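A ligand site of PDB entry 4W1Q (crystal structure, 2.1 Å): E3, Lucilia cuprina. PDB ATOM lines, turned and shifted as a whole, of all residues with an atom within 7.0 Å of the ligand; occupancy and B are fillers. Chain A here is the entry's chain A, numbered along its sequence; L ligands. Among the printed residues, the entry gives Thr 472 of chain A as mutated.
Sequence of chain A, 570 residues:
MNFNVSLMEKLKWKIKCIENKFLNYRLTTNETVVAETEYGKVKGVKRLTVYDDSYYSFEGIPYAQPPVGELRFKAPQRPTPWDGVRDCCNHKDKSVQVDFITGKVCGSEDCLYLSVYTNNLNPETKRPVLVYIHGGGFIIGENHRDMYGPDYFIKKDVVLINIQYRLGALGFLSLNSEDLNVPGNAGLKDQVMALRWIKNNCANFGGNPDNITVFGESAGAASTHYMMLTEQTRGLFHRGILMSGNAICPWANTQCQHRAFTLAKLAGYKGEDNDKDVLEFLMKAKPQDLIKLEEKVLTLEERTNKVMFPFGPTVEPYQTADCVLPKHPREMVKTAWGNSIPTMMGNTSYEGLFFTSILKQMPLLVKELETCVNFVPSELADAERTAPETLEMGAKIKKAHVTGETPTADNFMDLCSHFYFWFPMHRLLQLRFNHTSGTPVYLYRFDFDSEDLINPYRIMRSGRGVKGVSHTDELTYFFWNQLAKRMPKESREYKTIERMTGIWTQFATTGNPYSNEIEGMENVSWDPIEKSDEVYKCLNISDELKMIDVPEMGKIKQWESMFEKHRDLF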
ATOM      1  N   HIS A 134       7.460  15.331  22.976  1.00  0.00           N
ATOM      2  CA  HIS A 134       7.619  16.527  23.811  1.00  0.00           C
ATOM      3  C   HIS A 134       6.358  17.411  23.849  1.00  0.00           C
ATOM      4  O   HIS A 134       5.551  17.389  22.931  1.00  0.00           O
ATOM      5  CB  HIS A 134       8.815  17.346  23.342  1.00  0.00           C
ATOM      6  CG  HIS A 134       8.578  18.079  22.058  1.00  0.00           C
ATOM      7  ND1 HIS A 134       7.880  19.271  21.985  1.00  0.00           N
ATOM      8  CD2 HIS A 134       8.951  17.804  20.779  1.00  0.00           C
ATOM      9  CE1 HIS A 134       7.847  19.694  20.745  1.00  0.00           C
ATOM     10  NE2 HIS A 134       8.491  18.819  19.992  1.00  0.00           N
ATOM     11  N   GLY A 135       6.211  18.170  24.928  1.00  0.00           N
ATOM     12  CA  GLY A 135       5.111  19.119  25.034  1.00  0.00           C
ATOM     13  C   GLY A 135       5.574  20.489  24.589  1.00  0.00           C
ATOM     14  O   GLY A 135       6.589  20.590  23.891  1.00  0.00           O
ATOM     15  N   GLY A 136       4.845  21.524  25.000  1.00  0.00           N
ATOM     16  CA  GLY A 136       5.129  22.878  24.557  1.00  0.00           C
ATOM     17  C   GLY A 136       3.943  23.498  23.820  1.00  0.00           C
ATOM     18  O   GLY A 136       4.102  24.267  22.875  1.00  0.00           O
ATOM     19  N   GLY A 137       2.734  23.149  24.282  1.00  0.00           N
ATOM     20  CA  GLY A 137       1.499  23.719  23.774  1.00  0.00           C
ATOM     21  C   GLY A 137       1.286  23.596  22.270  1.00  0.00           C
ATOM     22  O   GLY A 137       0.478  24.312  21.707  1.00  0.00           O
ATOM     23  N   PHE A 138       2.029  22.683  21.636  1.00  0.00           N
ATOM     24  CA  PHE A 138       2.007  22.485  20.180  1.00  0.00           C
ATOM     25  C   PHE A 138       2.617  23.668  19.438  1.00  0.00           C
ATOM     26  O   PHE A 138       2.482  23.764  18.215  1.00  0.00           O
ATOM     27  CB  PHE A 138       0.581  22.244  19.662  1.00  0.00           C
ATOM     28  CG  PHE A 138      -0.046  20.977  20.142  1.00  0.00           C
ATOM     29  CD1 PHE A 138       0.399  19.749  19.680  1.00  0.00           C
ATOM     30  CD2 PHE A 138      -1.115  21.008  21.024  1.00  0.00           C
ATOM     31  CE1 PHE A 138      -0.203  18.579  20.110  1.00  0.00           C
ATOM     32  CE2 PHE A 138      -1.721  19.833  21.460  1.00  0.00           C
ATOM     33  CZ  PHE A 138      -1.271  18.617  20.998  1.00  0.00           C
ATOM     34  N   ILE A 140       5.977  25.135  20.765  1.00  0.00           N
ATOM     35  CA  ILE A 140       7.420  25.103  20.977  1.00  0.00           C
ATOM     36  C   ILE A 140       7.873  23.681  21.310  1.00  0.00           C
ATOM     37  O   ILE A 140       7.045  22.806  21.571  1.00  0.00           O
ATOM     38  CB  ILE A 140       7.900  26.048  22.133  1.00  0.00           C
ATOM     39  CG1 ILE A 140       7.402  25.561  23.498  1.00  0.00           C
ATOM     40  CG2 ILE A 140       7.533  27.500  21.879  1.00  0.00           C
ATOM     41  CD1 ILE A 140       8.152  26.140  24.651  1.00  0.00           C
ATOM     42  N   GLU A 217       4.372  14.600  27.887  1.00  0.00           N
ATOM     43  CA  GLU A 217       4.022  15.505  28.966  1.00  0.00           C
ATOM     44  C   GLU A 217       3.364  16.784  28.375  1.00  0.00           C
ATOM     45  O   GLU A 217       3.858  17.304  27.390  1.00  0.00           O
ATOM     46  CB  GLU A 217       5.296  15.801  29.772  1.00  0.00           C
ATOM     47  CG  GLU A 217       5.083  16.433  31.136  1.00  0.00           C
ATOM     48  CD  GLU A 217       5.199  17.939  31.091  1.00  0.00           C
ATOM     49  OE1 GLU A 217       5.996  18.449  30.278  1.00  0.00           O
ATOM     50  OE2 GLU A 217       4.480  18.615  31.852  1.00  0.00           O
ATOM     51  N   SER A 218       2.241  17.227  28.950  1.00  0.00           N
ATOM     52  CA  SER A 218       1.515  18.448  28.512  1.00  0.00           C
ATOM     53  C   SER A 218       0.858  18.306  27.108  1.00  0.00           C
ATOM     54  O   SER A 218      -0.029  17.481  26.901  1.00  0.00           O
ATOM     55  CB  SER A 218       2.473  19.660  28.543  1.00  0.00           C
ATOM     56  OG  SER A 218       1.812  20.893  28.313  1.00  0.00           O
ATOM     57  N   ALA A 219       1.288  19.132  26.140  1.00  0.00           N
ATOM     58  CA  ALA A 219       0.917  18.923  24.737  1.00  0.00           C
ATOM     59  C   ALA A 219       1.410  17.568  24.250  1.00  0.00           C
ATOM     60  O   ALA A 219       0.853  17.002  23.345  1.00  0.00           O
ATOM     61  CB  ALA A 219       1.516  20.045  23.841  1.00  0.00           C
ATOM     62  N   GLY A 220       2.496  17.071  24.850  1.00  0.00           N
ATOM     63  CA  GLY A 220       3.013  15.741  24.583  1.00  0.00           C
ATOM     64  C   GLY A 220       2.117  14.645  25.139  1.00  0.00           C
ATOM     65  O   GLY A 220       2.026  13.547  24.568  1.00  0.00           O
ATOM     66  N   ALA A 221       1.414  14.943  26.239  1.00  0.00           N
ATOM     67  CA  ALA A 221       0.455  14.011  26.814  1.00  0.00           C
ATOM     68  C   ALA A 221      -0.800  13.972  25.967  1.00  0.00           C
ATOM     69  O   ALA A 221      -1.334  12.898  25.701  1.00  0.00           O
ATOM     70  CB  ALA A 221       0.121  14.381  28.250  1.00  0.00           C
ATOM     71  N   SER A 244       0.353  14.690  32.896  1.00  0.00           N
ATOM     72  CA  SER A 244      -0.221  16.052  32.967  1.00  0.00           C
ATOM     73  C   SER A 244      -0.920  16.466  31.692  1.00  0.00           C
ATOM     74  O   SER A 244      -0.691  17.570  31.173  1.00  0.00           O
ATOM     75  CB  SER A 244       0.860  17.107  33.281  1.00  0.00           C
ATOM     76  OG  SER A 244       1.411  16.937  34.569  1.00  0.00           O
ATOM     77  N   TRP A 251      -7.326  23.143  26.397  1.00  0.00           N
ATOM     78  CA  TRP A 251      -6.296  23.706  25.531  1.00  0.00           C
ATOM     79  C   TRP A 251      -5.872  22.772  24.376  1.00  0.00           C
ATOM     80  O   TRP A 251      -5.108  23.179  23.504  1.00  0.00           O
ATOM     81  CB  TRP A 251      -5.049  24.055  26.362  1.00  0.00           C
ATOM     82  CG  TRP A 251      -4.703  22.964  27.317  1.00  0.00           C
ATOM     83  CD1 TRP A 251      -5.159  22.832  28.606  1.00  0.00           C
ATOM     84  CD2 TRP A 251      -3.870  21.827  27.062  1.00  0.00           C
ATOM     85  NE1 TRP A 251      -4.644  21.692  29.172  1.00  0.00           N
ATOM     86  CE2 TRP A 251      -3.844  21.052  28.249  1.00  0.00           C
ATOM     87  CE3 TRP A 251      -3.132  21.386  25.958  1.00  0.00           C
ATOM     88  CZ2 TRP A 251      -3.120  19.857  28.350  1.00  0.00           C
ATOM     89  CZ3 TRP A 251      -2.396  20.201  26.074  1.00  0.00           C
ATOM     90  CH2 TRP A 251      -2.403  19.451  27.258  1.00  0.00           C
ATOM     91  N   ALA A 252      -6.364  21.525  24.372  1.00  0.00           N
ATOM     92  CA  ALA A 252      -5.786  20.475  23.510  1.00  0.00           C
ATOM     93  C   ALA A 252      -6.480  20.289  22.163  1.00  0.00           C
ATOM     94  O   ALA A 252      -6.097  19.437  21.361  1.00  0.00           O
ATOM     95  CB  ALA A 252      -5.777  19.135  24.252  1.00  0.00           C
ATOM     96  N   MET A 308      -6.251  29.150  24.410  1.00  0.00           N
ATOM     97  CA  MET A 308      -4.860  29.327  24.768  1.00  0.00           C
ATOM     98  C   MET A 308      -3.968  29.548  23.543  1.00  0.00           C
ATOM     99  O   MET A 308      -3.074  30.396  23.546  1.00  0.00           O
ATOM    100  CB  MET A 308      -4.370  28.132  25.590  1.00  0.00           C
ATOM    101  CG  MET A 308      -3.139  28.450  26.429  1.00  0.00           C
ATOM    102  SD  MET A 308      -2.438  27.070  27.368  1.00  0.00           S
ATOM    103  CE  MET A 308      -3.565  26.966  28.748  1.00  0.00           C
ATOM    104  N   PHE A 309      -4.233  28.791  22.474  1.00  0.00           N
ATOM    105  CA  PHE A 309      -3.412  28.858  21.283  1.00  0.00           C
ATOM    106  C   PHE A 309      -4.280  29.001  20.028  1.00  0.00           C
ATOM    107  O   PHE A 309      -5.321  28.378  19.910  1.00  0.00           O
ATOM    108  CB  PHE A 309      -2.531  27.615  21.174  1.00  0.00           C
ATOM    109  CG  PHE A 309      -1.801  27.264  22.447  1.00  0.00           C
ATOM    110  CD1 PHE A 309      -0.691  28.000  22.856  1.00  0.00           C
ATOM    111  CD2 PHE A 309      -2.207  26.195  23.224  1.00  0.00           C
ATOM    112  CE1 PHE A 309       0.009  27.678  24.033  1.00  0.00           C
ATOM    113  CE2 PHE A 309      -1.500  25.861  24.397  1.00  0.00           C
ATOM    114  CZ  PHE A 309      -0.388  26.620  24.796  1.00  0.00           C
ATOM    115  N   PHE A 354       2.419  26.850  37.977  1.00  0.00           N
ATOM    116  CA  PHE A 354       3.007  27.304  36.729  1.00  0.00           C
ATOM    117  C   PHE A 354       2.649  28.742  36.369  1.00  0.00           C
ATOM    118  O   PHE A 354       3.497  29.510  35.921  1.00  0.00           O
ATOM    119  CB  PHE A 354       2.561  26.351  35.602  1.00  0.00           C
ATOM    120  CG  PHE A 354       3.239  26.603  34.294  1.00  0.00           C
ATOM    121  CD1 PHE A 354       2.695  27.491  33.381  1.00  0.00           C
ATOM    122  CD2 PHE A 354       4.425  25.962  33.988  1.00  0.00           C
ATOM    123  CE1 PHE A 354       3.330  27.726  32.160  1.00  0.00           C
ATOM    124  CE2 PHE A 354       5.075  26.190  32.786  1.00  0.00           C
ATOM    125  CZ  PHE A 354       4.520  27.076  31.863  1.00  0.00           C
ATOM    126  N   PHE A 355       1.389  29.118  36.561  1.00  0.00           N
ATOM    127  CA  PHE A 355       0.869  30.387  36.036  1.00  0.00           C
ATOM    128  C   PHE A 355       1.281  31.640  36.793  1.00  0.00           C
ATOM    129  O   PHE A 355       0.736  32.714  36.526  1.00  0.00           O
ATOM    130  CB  PHE A 355      -0.660  30.354  35.989  1.00  0.00           C
ATOM    131  CG  PHE A 355      -1.193  29.414  34.959  1.00  0.00           C
ATOM    132  CD1 PHE A 355      -1.349  29.824  33.644  1.00  0.00           C
ATOM    133  CD2 PHE A 355      -1.512  28.122  35.301  1.00  0.00           C
ATOM    134  CE1 PHE A 355      -1.822  28.959  32.698  1.00  0.00           C
ATOM    135  CE2 PHE A 355      -1.989  27.242  34.341  1.00  0.00           C
ATOM    136  CZ  PHE A 355      -2.141  27.666  33.040  1.00  0.00           C
ATOM    137  N   TYR A 420      -7.341  23.078  33.885  1.00  0.00           N
ATOM    138  CA  TYR A 420      -6.491  22.615  32.791  1.00  0.00           C
ATOM    139  C   TYR A 420      -6.110  21.113  32.857  1.00  0.00           C
ATOM    140  O   TYR A 420      -5.848  20.518  31.812  1.00  0.00           O
ATOM    141  CB  TYR A 420      -5.219  23.475  32.717  1.00  0.00           C
ATOM    142  CG  TYR A 420      -5.489  24.901  32.304  1.00  0.00           C
ATOM    143  CD1 TYR A 420      -5.959  25.197  31.025  1.00  0.00           C
ATOM    144  CD2 TYR A 420      -5.275  25.954  33.190  1.00  0.00           C
ATOM    145  CE1 TYR A 420      -6.231  26.515  30.639  1.00  0.00           C
ATOM    146  CE2 TYR A 420      -5.541  27.269  32.820  1.00  0.00           C
ATOM    147  CZ  TYR A 420      -6.008  27.548  31.544  1.00  0.00           C
ATOM    148  OH  TYR A 420      -6.257  28.854  31.179  1.00  0.00           O
ATOM    149  N   PHE A 421      -6.092  20.515  34.051  1.00  0.00           N
ATOM    150  CA  PHE A 421      -5.544  19.146  34.201  1.00  0.00           C
ATOM    151  C   PHE A 421      -6.434  18.114  34.940  1.00  0.00           C
ATOM    152  O   PHE A 421      -6.776  17.082  34.360  1.00  0.00           O
ATOM    153  CB  PHE A 421      -4.158  19.221  34.875  1.00  0.00           C
ATOM    154  CG  PHE A 421      -3.195  20.132  34.158  1.00  0.00           C
ATOM    155  CD1 PHE A 421      -2.638  19.753  32.943  1.00  0.00           C
ATOM    156  CD2 PHE A 421      -2.841  21.377  34.686  1.00  0.00           C
ATOM    157  CE1 PHE A 421      -1.761  20.582  32.276  1.00  0.00           C
ATOM    158  CE2 PHE A 421      -1.958  22.218  34.019  1.00  0.00           C
ATOM    159  CZ  PHE A 421      -1.422  21.818  32.803  1.00  0.00           C
ATOM    160  N   TYR A 457      12.104  25.044  31.932  1.00  0.00           N
ATOM    161  CA  TYR A 457      10.757  25.587  32.115  1.00  0.00           C
ATOM    162  C   TYR A 457      10.641  26.437  33.371  1.00  0.00           C
ATOM    163  O   TYR A 457       9.754  27.299  33.459  1.00  0.00           O
ATOM    164  CB  TYR A 457       9.721  24.471  32.166  1.00  0.00           C
ATOM    165  CG  TYR A 457       9.342  23.959  30.805  1.00  0.00           C
ATOM    166  CD1 TYR A 457       8.437  24.655  30.007  1.00  0.00           C
ATOM    167  CD2 TYR A 457       9.894  22.788  30.301  1.00  0.00           C
ATOM    168  CE1 TYR A 457       8.085  24.188  28.755  1.00  0.00           C
ATOM    169  CE2 TYR A 457       9.560  22.312  29.053  1.00  0.00           C
ATOM    170  CZ  TYR A 457       8.649  23.012  28.283  1.00  0.00           C
ATOM    171  OH  TYR A 457       8.307  22.548  27.040  1.00  0.00           O
ATOM    172  N   MET A 460      11.044  29.976  32.324  1.00  0.00           N
ATOM    173  CA  MET A 460       9.835  30.476  31.676  1.00  0.00           C
ATOM    174  C   MET A 460       8.748  30.894  32.683  1.00  0.00           C
ATOM    175  O   MET A 460       8.235  32.004  32.621  1.00  0.00           O
ATOM    176  CB  MET A 460       9.281  29.413  30.722  1.00  0.00           C
ATOM    177  CG  MET A 460       8.062  29.844  29.942  1.00  0.00           C
ATOM    178  SD  MET A 460       7.321  28.518  28.959  1.00  0.00           S
ATOM    179  CE  MET A 460       8.711  28.032  27.935  1.00  0.00           C
ATOM    180  N   HIS A 471       3.618  22.088  37.238  1.00  0.00           N
ATOM    181  CA  HIS A 471       3.615  21.475  35.907  1.00  0.00           C
ATOM    182  C   HIS A 471       5.025  21.568  35.298  1.00  0.00           C
ATOM    183  O   HIS A 471       5.645  22.636  35.357  1.00  0.00           O
ATOM    184  CB  HIS A 471       2.575  22.195  35.014  1.00  0.00           C
ATOM    185  CG  HIS A 471       2.431  21.601  33.652  1.00  0.00           C
ATOM    186  ND1 HIS A 471       2.839  22.262  32.510  1.00  0.00           N
ATOM    187  CD2 HIS A 471       1.937  20.410  33.234  1.00  0.00           C
ATOM    188  CE1 HIS A 471       2.594  21.503  31.452  1.00  0.00           C
ATOM    189  NE2 HIS A 471       2.059  20.372  31.869  1.00  0.00           N
ATOM    190  N   THR A 472       5.511  20.451  34.752  1.00  0.00           N
ATOM    191  CA  THR A 472       6.855  20.285  34.138  1.00  0.00           C
ATOM    192  C   THR A 472       8.027  20.069  35.101  1.00  0.00           C
ATOM    193  O   THR A 472       9.091  19.696  34.658  1.00  0.00           O
ATOM    194  CB  THR A 472       7.317  21.474  33.235  1.00  0.00           C
ATOM    195  OG1 THR A 472       7.714  22.586  34.056  1.00  0.00           O
ATOM    196  CG2 THR A 472       6.238  21.881  32.225  1.00  0.00           C
ATOM    197  N   LEU A 475       9.971  16.595  34.732  1.00  0.00           N
ATOM    198  CA  LEU A 475      10.826  16.286  33.592  1.00  0.00           C
ATOM    199  C   LEU A 475      12.279  16.221  34.013  1.00  0.00           C
ATOM    200  O   LEU A 475      13.116  15.562  33.397  1.00  0.00           O
ATOM    201  CB  LEU A 475      10.663  17.325  32.499  1.00  0.00           C
ATOM    202  CG  LEU A 475       9.313  17.334  31.800  1.00  0.00           C
ATOM    203  CD1 LEU A 475       9.252  18.467  30.789  1.00  0.00           C
ATOM    204  CD2 LEU A 475       9.084  15.971  31.144  1.00  0.00           C
HETATM  205  O1  LIG L   1       2.521  21.531  26.631  1.00  0.00           O
HETATM  206  P1  LIG L   1       2.392  22.262  27.943  1.00  0.00           P
HETATM  207  O2  LIG L   1       1.047  23.254  27.797  1.00  0.00           O
HETATM  208  C1  LIG L   1      -0.221  22.697  27.887  1.00  0.00           C
HETATM  209  C2  LIG L   1      -1.217  23.812  28.206  1.00  0.00           C
HETATM  210  O3  LIG L   1       3.619  23.365  27.874  1.00  0.00           O
HETATM  211  C3  LIG L   1       4.751  23.108  28.608  1.00  0.00           C
HETATM  212  C4  LIG L   1       4.721  23.964  29.852  1.00  0.00           C
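OG of Ser 218 is covalently linked to P1 of the ligand.
O1 of the ligand is in hydrogen-bond range of N of Ala 219 (2.7 Å).
An oxygen (O1) of the ligand sits at hydrogen-bond distance from the backbone NH (N) of Gly 136, 2.8 Å away.
O1 of the ligand sits at hydrogen-bond distance from N of Gly 137.
NE1 of Trp 251 lies within hydrogen-bond range of O of Tyr 420.
A ring nitrogen (NE2) of His 471 lies within hydrogen-bond range of the side-chain carboxylate of Glu 217 (3.0 Å).
C of Gly 135 touches O1 of the ligand (3.8 Å).
Trp 251 touches the ligand (CD2 to C2, 3.5 Å).
Met 308 touches the ligand (SD to C2, 3.6 Å).
Phe 354 touches the ligand.
Tyr 457 touches the ligand.
His 471 touches the ligand.
CG2 of Thr 472 touches C4 of the ligand (3.5 Å).
Hydrophobic or aromatic side chains that line the ligand: Ala 219, Trp 251, Met 308, Phe 354, Tyr 457 and His 471.
11 residues have an atom within 4 Å of the ligand: Gly 135, Gly 136, Gly 137, Ser 218, Ala 219, Trp 251, Met 308, Phe 354, Tyr 457, His 471 and Thr 472.
Along chain A the residues within 4 Å of the ligand span positions 135 to 472.
The nearest printed residue that does not touch the ligand is Phe 309 (4.3 Å).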
